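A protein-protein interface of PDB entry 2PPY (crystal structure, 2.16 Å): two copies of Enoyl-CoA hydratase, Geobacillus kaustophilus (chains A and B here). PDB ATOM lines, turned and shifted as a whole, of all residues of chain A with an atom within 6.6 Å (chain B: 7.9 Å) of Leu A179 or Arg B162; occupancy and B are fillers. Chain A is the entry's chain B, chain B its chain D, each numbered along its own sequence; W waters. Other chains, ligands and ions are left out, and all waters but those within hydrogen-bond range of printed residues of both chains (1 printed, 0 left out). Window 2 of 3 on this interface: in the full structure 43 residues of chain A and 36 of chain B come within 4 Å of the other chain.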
ATOM      1  N   ASP A 124     -23.335 -10.626  -1.735  1.00  0.00           N
ATOM      2  CA  ASP A 124     -21.904 -10.697  -2.035  1.00  0.00           C
ATOM      3  C   ASP A 124     -20.990 -10.384  -0.847  1.00  0.00           C
ATOM      4  O   ASP A 124     -19.899 -10.953  -0.719  1.00  0.00           O
ATOM      5  CB  ASP A 124     -21.559  -9.741  -3.182  1.00  0.00           C
ATOM      6  CG  ASP A 124     -22.453  -9.935  -4.389  1.00  0.00           C
ATOM      7  OD1 ASP A 124     -22.626 -11.095  -4.822  1.00  0.00           O
ATOM      8  OD2 ASP A 124     -22.978  -8.924  -4.906  1.00  0.00           O
ATOM      9  N   LEU A 125     -21.422  -9.459   0.001  1.00  0.00           N
ATOM     10  CA  LEU A 125     -20.641  -9.076   1.171  1.00  0.00           C
ATOM     11  C   LEU A 125     -21.547  -8.965   2.390  1.00  0.00           C
ATOM     12  O   LEU A 125     -22.754  -8.784   2.263  1.00  0.00           O
ATOM     13  CB  LEU A 125     -19.942  -7.733   0.931  1.00  0.00           C
ATOM     14  CG  LEU A 125     -18.903  -7.651  -0.195  1.00  0.00           C
ATOM     15  CD1 LEU A 125     -18.463  -6.208  -0.381  1.00  0.00           C
ATOM     16  CD2 LEU A 125     -17.710  -8.541   0.130  1.00  0.00           C
ATOM     17  N   ARG A 126     -20.947  -9.080   3.570  1.00  0.00           N
ATOM     18  CA  ARG A 126     -21.672  -8.986   4.828  1.00  0.00           C
ATOM     19  C   ARG A 126     -20.839  -8.181   5.834  1.00  0.00           C
ATOM     20  O   ARG A 126     -19.709  -8.557   6.156  1.00  0.00           O
ATOM     21  CB  ARG A 126     -21.949 -10.395   5.376  1.00  0.00           C
ATOM     22  CG  ARG A 126     -23.020 -11.184   4.608  1.00  0.00           C
ATOM     23  CD  ARG A 126     -22.893 -12.680   4.866  1.00  0.00           C
ATOM     24  NE  ARG A 126     -21.677 -13.191   4.241  1.00  0.00           N
ATOM     25  CZ  ARG A 126     -21.539 -13.363   2.929  1.00  0.00           C
ATOM     26  NH1 ARG A 126     -22.548 -13.076   2.119  1.00  0.00           N
ATOM     27  NH2 ARG A 126     -20.383 -13.778   2.424  1.00  0.00           N
ATOM     28  N   LEU A 157     -18.927 -21.119   2.090  1.00  0.00           N
ATOM     29  CA  LEU A 157     -18.336 -19.908   2.645  1.00  0.00           C
ATOM     30  C   LEU A 157     -17.355 -20.172   3.787  1.00  0.00           C
ATOM     31  O   LEU A 157     -16.233 -19.665   3.765  1.00  0.00           O
ATOM     32  CB  LEU A 157     -19.436 -18.955   3.122  1.00  0.00           C
ATOM     33  CG  LEU A 157     -18.973 -17.634   3.746  1.00  0.00           C
ATOM     34  CD1 LEU A 157     -18.226 -16.804   2.716  1.00  0.00           C
ATOM     35  CD2 LEU A 157     -20.180 -16.864   4.253  1.00  0.00           C
ATOM     36  N   ILE A 173     -23.462 -17.819  16.773  1.00  0.00           N
ATOM     37  CA  ILE A 173     -22.206 -17.243  17.233  1.00  0.00           C
ATOM     38  C   ILE A 173     -22.243 -15.720  17.237  1.00  0.00           C
ATOM     39  O   ILE A 173     -23.182 -15.107  16.719  1.00  0.00           O
ATOM     40  CB  ILE A 173     -21.030 -17.714  16.343  1.00  0.00           C
ATOM     41  CG1 ILE A 173     -21.206 -17.184  14.916  1.00  0.00           C
ATOM     42  CG2 ILE A 173     -20.965 -19.237  16.344  1.00  0.00           C
ATOM     43  CD1 ILE A 173     -20.118 -17.619  13.946  1.00  0.00           C
ATOM     44  N   THR A 174     -21.207 -15.123  17.824  1.00  0.00           N
ATOM     45  CA  THR A 174     -21.080 -13.672  17.921  1.00  0.00           C
ATOM     46  C   THR A 174     -20.522 -13.102  16.622  1.00  0.00           C
ATOM     47  O   THR A 174     -20.041 -13.844  15.764  1.00  0.00           O
ATOM     48  CB  THR A 174     -20.114 -13.266  19.060  1.00  0.00           C
ATOM     49  OG1 THR A 174     -18.775 -13.635  18.698  1.00  0.00           O
ATOM     50  CG2 THR A 174     -20.491 -13.963  20.369  1.00  0.00           C
ATOM     51  N   PRO A 175     -20.577 -11.770  16.462  1.00  0.00           N
ATOM     52  CA  PRO A 175     -20.060 -11.128  15.252  1.00  0.00           C
ATOM     53  C   PRO A 175     -18.553 -11.330  15.122  1.00  0.00           C
ATOM     54  O   PRO A 175     -18.040 -11.564  14.024  1.00  0.00           O
ATOM     55  CB  PRO A 175     -20.422  -9.661  15.461  1.00  0.00           C
ATOM     56  CG  PRO A 175     -21.675  -9.738  16.277  1.00  0.00           C
ATOM     57  CD  PRO A 175     -21.326 -10.805  17.284  1.00  0.00           C
ATOM     58  N   GLN A 176     -17.849 -11.234  16.248  1.00  0.00           N
ATOM     59  CA  GLN A 176     -16.396 -11.402  16.261  1.00  0.00           C
ATOM     60  C   GLN A 176     -16.000 -12.795  15.769  1.00  0.00           C
ATOM     61  O   GLN A 176     -15.037 -12.950  15.012  1.00  0.00           O
ATOM     62  CB  GLN A 176     -15.843 -11.173  17.671  1.00  0.00           C
ATOM     63  CG  GLN A 176     -15.971  -9.740  18.196  1.00  0.00           C
ATOM     64  CD  GLN A 176     -17.408  -9.320  18.478  1.00  0.00           C
ATOM     65  OE1 GLN A 176     -18.185 -10.073  19.062  1.00  0.00           O
ATOM     66  NE2 GLN A 176     -17.757  -8.104  18.078  1.00  0.00           N
ATOM     67  N   GLU A 177     -16.750 -13.802  16.205  1.00  0.00           N
ATOM     68  CA  GLU A 177     -16.502 -15.185  15.814  1.00  0.00           C
ATOM     69  C   GLU A 177     -16.837 -15.391  14.342  1.00  0.00           C
ATOM     70  O   GLU A 177     -16.188 -16.176  13.652  1.00  0.00           O
ATOM     71  CB  GLU A 177     -17.346 -16.129  16.670  1.00  0.00           C
ATOM     72  CG  GLU A 177     -16.849 -16.274  18.096  1.00  0.00           C
ATOM     73  CD  GLU A 177     -17.889 -16.873  19.022  1.00  0.00           C
ATOM     74  OE1 GLU A 177     -17.506 -17.361  20.107  1.00  0.00           O
ATOM     75  OE2 GLU A 177     -19.088 -16.845  18.673  1.00  0.00           O
ATOM     76  N   ALA A 178     -17.859 -14.689  13.868  1.00  0.00           N
ATOM     77  CA  ALA A 178     -18.263 -14.790  12.475  1.00  0.00           C
ATOM     78  C   ALA A 178     -17.135 -14.270  11.592  1.00  0.00           C
ATOM     79  O   ALA A 178     -16.809 -14.867  10.567  1.00  0.00           O
ATOM     80  CB  ALA A 178     -19.529 -13.984  12.240  1.00  0.00           C
ATOM     81  N   LEU A 179     -16.535 -13.160  12.002  1.00  0.00           N
ATOM     82  CA  LEU A 179     -15.443 -12.556  11.248  1.00  0.00           C
ATOM     83  C   LEU A 179     -14.256 -13.510  11.155  1.00  0.00           C
ATOM     84  O   LEU A 179     -13.623 -13.642  10.103  1.00  0.00           O
ATOM     85  CB  LEU A 179     -14.996 -11.257  11.927  1.00  0.00           C
ATOM     86  CG  LEU A 179     -13.936 -10.433  11.197  1.00  0.00           C
ATOM     87  CD1 LEU A 179     -14.512  -9.914   9.887  1.00  0.00           C
ATOM     88  CD2 LEU A 179     -13.489  -9.274  12.075  1.00  0.00           C
ATOM     89  N   GLU A 180     -13.967 -14.176  12.267  1.00  0.00           N
ATOM     90  CA  GLU A 180     -12.855 -15.111  12.348  1.00  0.00           C
ATOM     91  C   GLU A 180     -12.993 -16.312  11.412  1.00  0.00           C
ATOM     92  O   GLU A 180     -12.003 -16.770  10.840  1.00  0.00           O
ATOM     93  CB  GLU A 180     -12.693 -15.582  13.795  1.00  0.00           C
ATOM     94  CG  GLU A 180     -11.474 -16.442  14.052  1.00  0.00           C
ATOM     95  CD  GLU A 180     -11.130 -16.521  15.529  1.00  0.00           C
ATOM     96  OE1 GLU A 180     -12.006 -16.925  16.327  1.00  0.00           O
ATOM     97  OE2 GLU A 180      -9.986 -16.178  15.894  1.00  0.00           O
ATOM     98  N   ILE A 181     -14.209 -16.827  11.249  1.00  0.00           N
ATOM     99  CA  ILE A 181     -14.405 -17.973  10.367  1.00  0.00           C
ATOM    100  C   ILE A 181     -14.784 -17.559   8.946  1.00  0.00           C
ATOM    101  O   ILE A 181     -15.070 -18.405   8.105  1.00  0.00           O
ATOM    102  CB  ILE A 181     -15.478 -18.948  10.921  1.00  0.00           C
ATOM    103  CG1 ILE A 181     -16.838 -18.260  10.996  1.00  0.00           C
ATOM    104  CG2 ILE A 181     -15.068 -19.434  12.308  1.00  0.00           C
ATOM    105  CD1 ILE A 181     -17.941 -19.160  11.507  1.00  0.00           C
ATOM    106  N   GLY A 182     -14.774 -16.256   8.684  1.00  0.00           N
ATOM    107  CA  GLY A 182     -15.109 -15.762   7.360  1.00  0.00           C
ATOM    108  C   GLY A 182     -16.600 -15.721   7.062  1.00  0.00           C
ATOM    109  O   GLY A 182     -17.001 -15.634   5.901  1.00  0.00           O
ATOM    110  N   LEU A 183     -17.427 -15.781   8.103  1.00  0.00           N
ATOM    111  CA  LEU A 183     -18.872 -15.740   7.926  1.00  0.00           C
ATOM    112  C   LEU A 183     -19.267 -14.333   7.485  1.00  0.00           C
ATOM    113  O   LEU A 183     -20.248 -14.151   6.770  1.00  0.00           O
ATOM    114  CB  LEU A 183     -19.587 -16.092   9.232  1.00  0.00           C
ATOM    115  CG  LEU A 183     -20.882 -16.908   9.107  1.00  0.00           C
ATOM    116  CD1 LEU A 183     -21.621 -16.872  10.434  1.00  0.00           C
ATOM    117  CD2 LEU A 183     -21.769 -16.355   8.002  1.00  0.00           C
ATOM    118  N   VAL A 184     -18.509 -13.336   7.934  1.00  0.00           N
ATOM    119  CA  VAL A 184     -18.765 -11.954   7.545  1.00  0.00           C
ATOM    120  C   VAL A 184     -17.455 -11.345   7.064  1.00  0.00           C
ATOM    121  O   VAL A 184     -16.379 -11.855   7.373  1.00  0.00           O
ATOM    122  CB  VAL A 184     -19.335 -11.102   8.716  1.00  0.00           C
ATOM    123  CG1 VAL A 184     -20.645 -11.701   9.196  1.00  0.00           C
ATOM    124  CG2 VAL A 184     -18.329 -11.014   9.859  1.00  0.00           C
ATOM    125  N   ASN A 185     -17.551 -10.262   6.302  1.00  0.00           N
ATOM    126  CA  ASN A 185     -16.377  -9.593   5.756  1.00  0.00           C
ATOM    127  C   ASN A 185     -15.828  -8.492   6.655  1.00  0.00           C
ATOM    128  O   ASN A 185     -14.642  -8.172   6.596  1.00  0.00           O
ATOM    129  CB  ASN A 185     -16.723  -8.996   4.394  1.00  0.00           C
ATOM    130  CG  ASN A 185     -17.114 -10.047   3.385  1.00  0.00           C
ATOM    131  OD1 ASN A 185     -16.264 -10.597   2.687  1.00  0.00           O
ATOM    132  ND2 ASN A 185     -18.404 -10.347   3.316  1.00  0.00           N
ATOM    133  N   ARG A 186     -16.694  -7.900   7.469  1.00  0.00           N
ATOM    134  CA  ARG A 186     -16.282  -6.826   8.363  1.00  0.00           C
ATOM    135  C   ARG A 186     -17.112  -6.805   9.633  1.00  0.00           C
ATOM    136  O   ARG A 186     -18.207  -7.364   9.695  1.00  0.00           O
ATOM    137  CB  ARG A 186     -16.441  -5.459   7.686  1.00  0.00           C
ATOM    138  CG  ARG A 186     -15.651  -5.246   6.407  1.00  0.00           C
ATOM    139  CD  ARG A 186     -14.239  -4.767   6.669  1.00  0.00           C
ATOM    140  NE  ARG A 186     -13.653  -4.200   5.458  1.00  0.00           N
ATOM    141  CZ  ARG A 186     -13.388  -4.899   4.359  1.00  0.00           C
ATOM    142  NH1 ARG A 186     -12.860  -4.299   3.298  1.00  0.00           N
ATOM    143  NH2 ARG A 186     -13.637  -6.202   4.328  1.00  0.00           N
ATOM    144  N   VAL A 187     -16.560  -6.153  10.646  1.00  0.00           N
ATOM    145  CA  VAL A 187     -17.225  -5.964  11.922  1.00  0.00           C
ATOM    146  C   VAL A 187     -16.886  -4.534  12.297  1.00  0.00           C
ATOM    147  O   VAL A 187     -15.721  -4.194  12.510  1.00  0.00           O
ATOM    148  CB  VAL A 187     -16.717  -6.928  13.002  1.00  0.00           C
ATOM    149  CG1 VAL A 187     -17.157  -6.436  14.374  1.00  0.00           C
ATOM    150  CG2 VAL A 187     -17.281  -8.326  12.755  1.00  0.00           C
ATOM    151  N   LEU B 154      -7.732 -16.384  -6.933  1.00  0.00           N
ATOM    152  CA  LEU B 154      -7.807 -15.750  -5.619  1.00  0.00           C
ATOM    153  C   LEU B 154      -9.041 -16.250  -4.880  1.00  0.00           C
ATOM    154  O   LEU B 154      -8.984 -16.548  -3.685  1.00  0.00           O
ATOM    155  CB  LEU B 154      -7.869 -14.222  -5.719  1.00  0.00           C
ATOM    156  CG  LEU B 154      -7.700 -13.557  -4.339  1.00  0.00           C
ATOM    157  CD1 LEU B 154      -6.281 -13.811  -3.844  1.00  0.00           C
ATOM    158  CD2 LEU B 154      -7.968 -12.062  -4.410  1.00  0.00           C
ATOM    159  N   ALA B 155     -10.157 -16.348  -5.597  1.00  0.00           N
ATOM    160  CA  ALA B 155     -11.406 -16.818  -5.001  1.00  0.00           C
ATOM    161  C   ALA B 155     -11.254 -18.229  -4.452  1.00  0.00           C
ATOM    162  O   ALA B 155     -11.715 -18.540  -3.352  1.00  0.00           O
ATOM    163  CB  ALA B 155     -12.526 -16.786  -6.037  1.00  0.00           C
ATOM    164  N   LEU B 157      -8.406 -19.715  -3.639  1.00  0.00           N
ATOM    165  CA  LEU B 157      -7.386 -19.771  -2.591  1.00  0.00           C
ATOM    166  C   LEU B 157      -7.809 -19.203  -1.236  1.00  0.00           C
ATOM    167  O   LEU B 157      -7.628 -19.855  -0.207  1.00  0.00           O
ATOM    168  CB  LEU B 157      -6.108 -19.058  -3.053  1.00  0.00           C
ATOM    169  CG  LEU B 157      -4.873 -19.175  -2.155  1.00  0.00           C
ATOM    170  CD1 LEU B 157      -4.449 -20.635  -2.050  1.00  0.00           C
ATOM    171  CD2 LEU B 157      -3.727 -18.340  -2.732  1.00  0.00           C
ATOM    172  N   ILE B 158      -8.376 -17.999  -1.226  1.00  0.00           N
ATOM    173  CA  ILE B 158      -8.764 -17.377   0.032  1.00  0.00           C
ATOM    174  C   ILE B 158     -10.263 -17.289   0.300  1.00  0.00           C
ATOM    175  O   ILE B 158     -10.677 -16.764   1.334  1.00  0.00           O
ATOM    176  CB  ILE B 158      -8.167 -15.951   0.154  1.00  0.00           C
ATOM    177  CG1 ILE B 158      -8.884 -14.990  -0.795  1.00  0.00           C
ATOM    178  CG2 ILE B 158      -6.670 -15.980  -0.163  1.00  0.00           C
ATOM    179  CD1 ILE B 158      -8.558 -13.523  -0.528  1.00  0.00           C
ATOM    180  N   GLY B 159     -11.075 -17.812  -0.615  1.00  0.00           N
ATOM    181  CA  GLY B 159     -12.516 -17.758  -0.436  1.00  0.00           C
ATOM    182  C   GLY B 159     -13.102 -16.732  -1.389  1.00  0.00           C
ATOM    183  O   GLY B 159     -12.532 -15.649  -1.567  1.00  0.00           O
ATOM    184  N   TYR B 160     -14.243 -17.057  -1.991  1.00  0.00           N
ATOM    185  CA  TYR B 160     -14.874 -16.164  -2.956  1.00  0.00           C
ATOM    186  C   TYR B 160     -15.322 -14.790  -2.457  1.00  0.00           C
ATOM    187  O   TYR B 160     -15.244 -13.818  -3.204  1.00  0.00           O
ATOM    188  CB  TYR B 160     -16.049 -16.875  -3.639  1.00  0.00           C
ATOM    189  CG  TYR B 160     -17.167 -17.315  -2.718  1.00  0.00           C
ATOM    190  CD1 TYR B 160     -18.233 -16.458  -2.412  1.00  0.00           C
ATOM    191  CD2 TYR B 160     -17.185 -18.603  -2.186  1.00  0.00           C
ATOM    192  CE1 TYR B 160     -19.289 -16.883  -1.606  1.00  0.00           C
ATOM    193  CE2 TYR B 160     -18.232 -19.034  -1.383  1.00  0.00           C
ATOM    194  CZ  TYR B 160     -19.284 -18.175  -1.100  1.00  0.00           C
ATOM    195  OH  TYR B 160     -20.336 -18.634  -0.338  1.00  0.00           O
ATOM    196  N   SER B 161     -15.783 -14.689  -1.216  1.00  0.00           N
ATOM    197  CA  SER B 161     -16.232 -13.394  -0.706  1.00  0.00           C
ATOM    198  C   SER B 161     -15.061 -12.461  -0.397  1.00  0.00           C
ATOM    199  O   SER B 161     -15.111 -11.270  -0.704  1.00  0.00           O
ATOM    200  CB  SER B 161     -17.096 -13.567   0.543  1.00  0.00           C
ATOM    201  OG  SER B 161     -17.685 -12.326   0.915  1.00  0.00           O
ATOM    202  N   ARG B 162     -14.015 -13.002   0.218  1.00  0.00           N
ATOM    203  CA  ARG B 162     -12.828 -12.213   0.530  1.00  0.00           C
ATOM    204  C   ARG B 162     -12.154 -11.799  -0.769  1.00  0.00           C
ATOM    205  O   ARG B 162     -11.674 -10.673  -0.900  1.00  0.00           O
ATOM    206  CB  ARG B 162     -11.842 -13.026   1.374  1.00  0.00           C
ATOM    207  CG  ARG B 162     -12.307 -13.243   2.801  1.00  0.00           C
ATOM    208  CD  ARG B 162     -11.298 -14.031   3.615  1.00  0.00           C
ATOM    209  NE  ARG B 162     -11.714 -14.105   5.011  1.00  0.00           N
ATOM    210  CZ  ARG B 162     -11.013 -14.690   5.978  1.00  0.00           C
ATOM    211  NH1 ARG B 162      -9.850 -15.260   5.703  1.00  0.00           N
ATOM    212  NH2 ARG B 162     -11.473 -14.693   7.222  1.00  0.00           N
ATOM    213  N   ALA B 163     -12.119 -12.718  -1.730  1.00  0.00           N
ATOM    214  CA  ALA B 163     -11.506 -12.425  -3.019  1.00  0.00           C
ATOM    215  C   ALA B 163     -12.311 -11.337  -3.737  1.00  0.00           C
ATOM    216  O   ALA B 163     -11.744 -10.445  -4.371  1.00  0.00           O
ATOM    217  CB  ALA B 163     -11.446 -13.681  -3.864  1.00  0.00           C
ATOM    218  N   LEU B 164     -13.634 -11.406  -3.630  1.00  0.00           N
ATOM    219  CA  LEU B 164     -14.486 -10.412  -4.268  1.00  0.00           C
ATOM    220  C   LEU B 164     -14.194  -9.029  -3.678  1.00  0.00           C
ATOM    221  O   LEU B 164     -13.981  -8.058  -4.410  1.00  0.00           O
ATOM    222  CB  LEU B 164     -15.959 -10.781  -4.079  1.00  0.00           C
ATOM    223  CG  LEU B 164     -16.978  -9.841  -4.733  1.00  0.00           C
ATOM    224  CD1 LEU B 164     -18.116 -10.655  -5.323  1.00  0.00           C
ATOM    225  CD2 LEU B 164     -17.500  -8.848  -3.708  1.00  0.00           C
ATOM    226  N   ASP B 165     -14.174  -8.957  -2.351  1.00  0.00           N
ATOM    227  CA  ASP B 165     -13.890  -7.717  -1.633  1.00  0.00           C
ATOM    228  C   ASP B 165     -12.570  -7.105  -2.109  1.00  0.00           C
ATOM    229  O   ASP B 165     -12.523  -5.929  -2.474  1.00  0.00           O
ATOM    230  CB  ASP B 165     -13.851  -8.013  -0.127  1.00  0.00           C
ATOM    231  CG  ASP B 165     -13.302  -6.855   0.701  1.00  0.00           C
ATOM    232  OD1 ASP B 165     -13.497  -5.676   0.327  1.00  0.00           O
ATOM    233  OD2 ASP B 165     -12.687  -7.138   1.752  1.00  0.00           O
ATOM    234  N   MET B 166     -11.508  -7.909  -2.127  1.00  0.00           N
ATOM    235  CA  MET B 166     -10.192  -7.440  -2.557  1.00  0.00           C
ATOM    236  C   MET B 166     -10.143  -7.015  -4.023  1.00  0.00           C
ATOM    237  O   MET B 166      -9.426  -6.081  -4.381  1.00  0.00           O
ATOM    238  CB  MET B 166      -9.126  -8.519  -2.324  1.00  0.00           C
ATOM    239  CG  MET B 166      -8.730  -8.738  -0.868  1.00  0.00           C
ATOM    240  SD  MET B 166      -7.177  -9.904  -0.691  1.00  0.00           S
ATOM    241  CE  MET B 166      -5.822  -8.707  -1.345  1.00  0.00           C
ATOM    242  N   ASN B 167     -10.892  -7.709  -4.869  1.00  0.00           N
ATOM    243  CA  ASN B 167     -10.910  -7.392  -6.293  1.00  0.00           C
ATOM    244  C   ASN B 167     -11.693  -6.124  -6.625  1.00  0.00           C
ATOM    245  O   ASN B 167     -11.226  -5.286  -7.391  1.00  0.00           O
ATOM    246  CB  ASN B 167     -11.487  -8.571  -7.091  1.00  0.00           C
ATOM    247  CG  ASN B 167     -10.435  -9.605  -7.452  1.00  0.00           C
ATOM    248  OD1 ASN B 167      -9.715  -9.457  -8.444  1.00  0.00           O
ATOM    249  ND2 ASN B 167     -10.329 -10.653  -6.638  1.00  0.00           N
ATOM    250  N   ILE B 168     -12.883  -5.980  -6.055  1.00  0.00           N
ATOM    251  CA  ILE B 168     -13.692  -4.804  -6.346  1.00  0.00           C
ATOM    252  C   ILE B 168     -13.122  -3.493  -5.788  1.00  0.00           C
ATOM    253  O   ILE B 168     -13.354  -2.430  -6.361  1.00  0.00           O
ATOM    254  CB  ILE B 168     -15.140  -4.986  -5.852  1.00  0.00           C
ATOM    255  CG1 ILE B 168     -15.176  -5.109  -4.330  1.00  0.00           C
ATOM    256  CG2 ILE B 168     -15.753  -6.224  -6.516  1.00  0.00           C
ATOM    257  CD1 ILE B 168     -16.583  -5.140  -3.783  1.00  0.00           C
ATOM    258  N   THR B 169     -12.370  -3.569  -4.692  1.00  0.00           N
ATOM    259  CA  THR B 169     -11.778  -2.371  -4.090  1.00  0.00           C
ATOM    260  C   THR B 169     -10.387  -2.109  -4.652  1.00  0.00           C
ATOM    261  O   THR B 169      -9.939  -0.964  -4.709  1.00  0.00           O
ATOM    262  CB  THR B 169     -11.658  -2.485  -2.546  1.00  0.00           C
ATOM    263  OG1 THR B 169     -10.692  -3.488  -2.209  1.00  0.00           O
ATOM    264  CG2 THR B 169     -13.006  -2.843  -1.924  1.00  0.00           C
ATOM    265  N   GLU B 177      -0.801 -10.039   6.612  1.00  0.00           N
ATOM    266  CA  GLU B 177      -2.228 -10.169   6.352  1.00  0.00           C
ATOM    267  C   GLU B 177      -2.414 -11.242   5.279  1.00  0.00           C
ATOM    268  O   GLU B 177      -3.355 -12.030   5.328  1.00  0.00           O
ATOM    269  CB  GLU B 177      -2.818  -8.839   5.877  1.00  0.00           C
ATOM    270  CG  GLU B 177      -2.863  -7.766   6.953  1.00  0.00           C
ATOM    271  CD  GLU B 177      -3.464  -6.459   6.463  1.00  0.00           C
ATOM    272  OE1 GLU B 177      -2.923  -5.877   5.500  1.00  0.00           O
ATOM    273  OE2 GLU B 177      -4.477  -6.013   7.042  1.00  0.00           O
ATOM    274  N   GLU B 180      -2.220 -14.750   6.969  1.00  0.00           N
ATOM    275  CA  GLU B 180      -3.391 -15.159   7.734  1.00  0.00           C
ATOM    276  C   GLU B 180      -4.605 -15.570   6.914  1.00  0.00           C
ATOM    277  O   GLU B 180      -5.378 -16.423   7.348  1.00  0.00           O
ATOM    278  CB  GLU B 180      -3.775 -14.078   8.744  1.00  0.00           C
ATOM    279  CG  GLU B 180      -3.673 -12.654   8.254  1.00  0.00           C
ATOM    280  CD  GLU B 180      -3.827 -11.663   9.395  1.00  0.00           C
ATOM    281  OE1 GLU B 180      -3.690 -10.443   9.160  1.00  0.00           O
ATOM    282  OE2 GLU B 180      -4.086 -12.110  10.533  1.00  0.00           O
ATOM    283  N   ILE B 181      -4.782 -14.980   5.736  1.00  0.00           N
ATOM    284  CA  ILE B 181      -5.919 -15.358   4.905  1.00  0.00           C
ATOM    285  C   ILE B 181      -5.578 -16.517   3.961  1.00  0.00           C
ATOM    286  O   ILE B 181      -6.436 -17.004   3.220  1.00  0.00           O
ATOM    287  CB  ILE B 181      -6.458 -14.153   4.095  1.00  0.00           C
ATOM    288  CG1 ILE B 181      -5.373 -13.579   3.191  1.00  0.00           C
ATOM    289  CG2 ILE B 181      -6.949 -13.078   5.049  1.00  0.00           C
ATOM    290  CD1 ILE B 181      -5.870 -12.441   2.333  1.00  0.00           C
ATOM    291  N   GLY B 182      -4.324 -16.963   4.004  1.00  0.00           N
ATOM    292  CA  GLY B 182      -3.894 -18.067   3.164  1.00  0.00           C
ATOM    293  C   GLY B 182      -3.402 -17.673   1.783  1.00  0.00           C
ATOM    294  O   GLY B 182      -3.256 -18.532   0.907  1.00  0.00           O
HETATM  295  O   HOH W   1     -13.484  -9.424   3.100  1.00  0.00           O
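5 positions are printed for both chains. Of the 10 pairs that touch across the chains among the printed residues, none has its exchanged pair printed and touching as well.
The backbone NH (N) of Arg A186 lies within hydrogen-bond range of the backbone carbonyl oxygen (O) of Arg A126 (3.4 Å). The backbone carbonyl oxygen (O) of Arg A126 sits at hydrogen-bond distance from the backbone NH (N) of Asn A185 (2.8 Å). The backbone carbonyl oxygen (O) of Leu A183 sits at hydrogen-bond distance from the guanidinium group (NE) of Arg A126 (3.1 Å). The backbone carbonyl oxygen (O) of Asp B165 lies within hydrogen-bond range of the side-chain hydroxyl (OG1) of Thr B169, 3.1 Å away. The backbone NH of Tyr B160 sits at hydrogen-bond distance from the backbone carbonyl oxygen of Ala B155.
OG of Ser B161 lies within hydrogen-bond range of O of Asp A124 (3.1 Å). The side-chain amide oxygen of Asn A185 lies within hydrogen-bond range of the side-chain hydroxyl of Ser B161, 2.9 Å away. NH2 of Arg A186 is in salt-bridge range of OD2 of Asp B165 (2.9 Å). The guanidinium group of Arg A126 is in hydrogen-bond range of the side-chain hydroxyl of Ser B161.
Leu A179 touches just one residue of chain B: Arg B162. Arg B162 touches just these residues of chain A: Leu A179 (3.7 Å) and Gly A182 (3.8 Å). Of the printed residues of chain A, Leu B164 touches Leu A125. Of the printed residues of chain A, Asp B165 touches Leu A125 and Arg A186. Printed residues of chain B within 4 Å of Asn A185: Ser B161 (2.9 Å). Of the printed residues of chain B, Arg A126 touches Ser B161. Leu A183 touches none of the printed residues of chain B. Met B166 touches none of the printed residues of chain A. The nearest printed residue of chain B that does not touch Leu A179 is Ile B181 (8.4 Å).
Water W1 lies within hydrogen-bond range of the side-chain carboxylate of Asp B165 (2.8 Å), the side-chain amide oxygen of Asn A185 (3.0 Å) and the guanidinium group of Arg A186 (3.5 Å).
Among the printed residues, merely in contact across the chains: Leu A125 with Ser B161 (3.9 Å), Leu A125 with Leu B164 (3.9 Å), Leu A125 with Asp B165 (3.9 Å), Leu A157 with Tyr B160 (3.6 Å), Leu A179 with Arg B162 (3.7 Å) and Gly A182 with Arg B162 (3.8 Å).
Hydrophobic or aromatic side chains of chain B within 4 Å of the printed part of chain A: Tyr B160 and Leu B164. Of the 19 printed residues of chain A, 8 touch a printed residue of chain B. Printed residues of chain A that touch a printed residue of chain B: Asp A124, Leu A125, Arg A126, Leu A157, Leu A179, Gly A182, Asn A185 and Arg A186.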
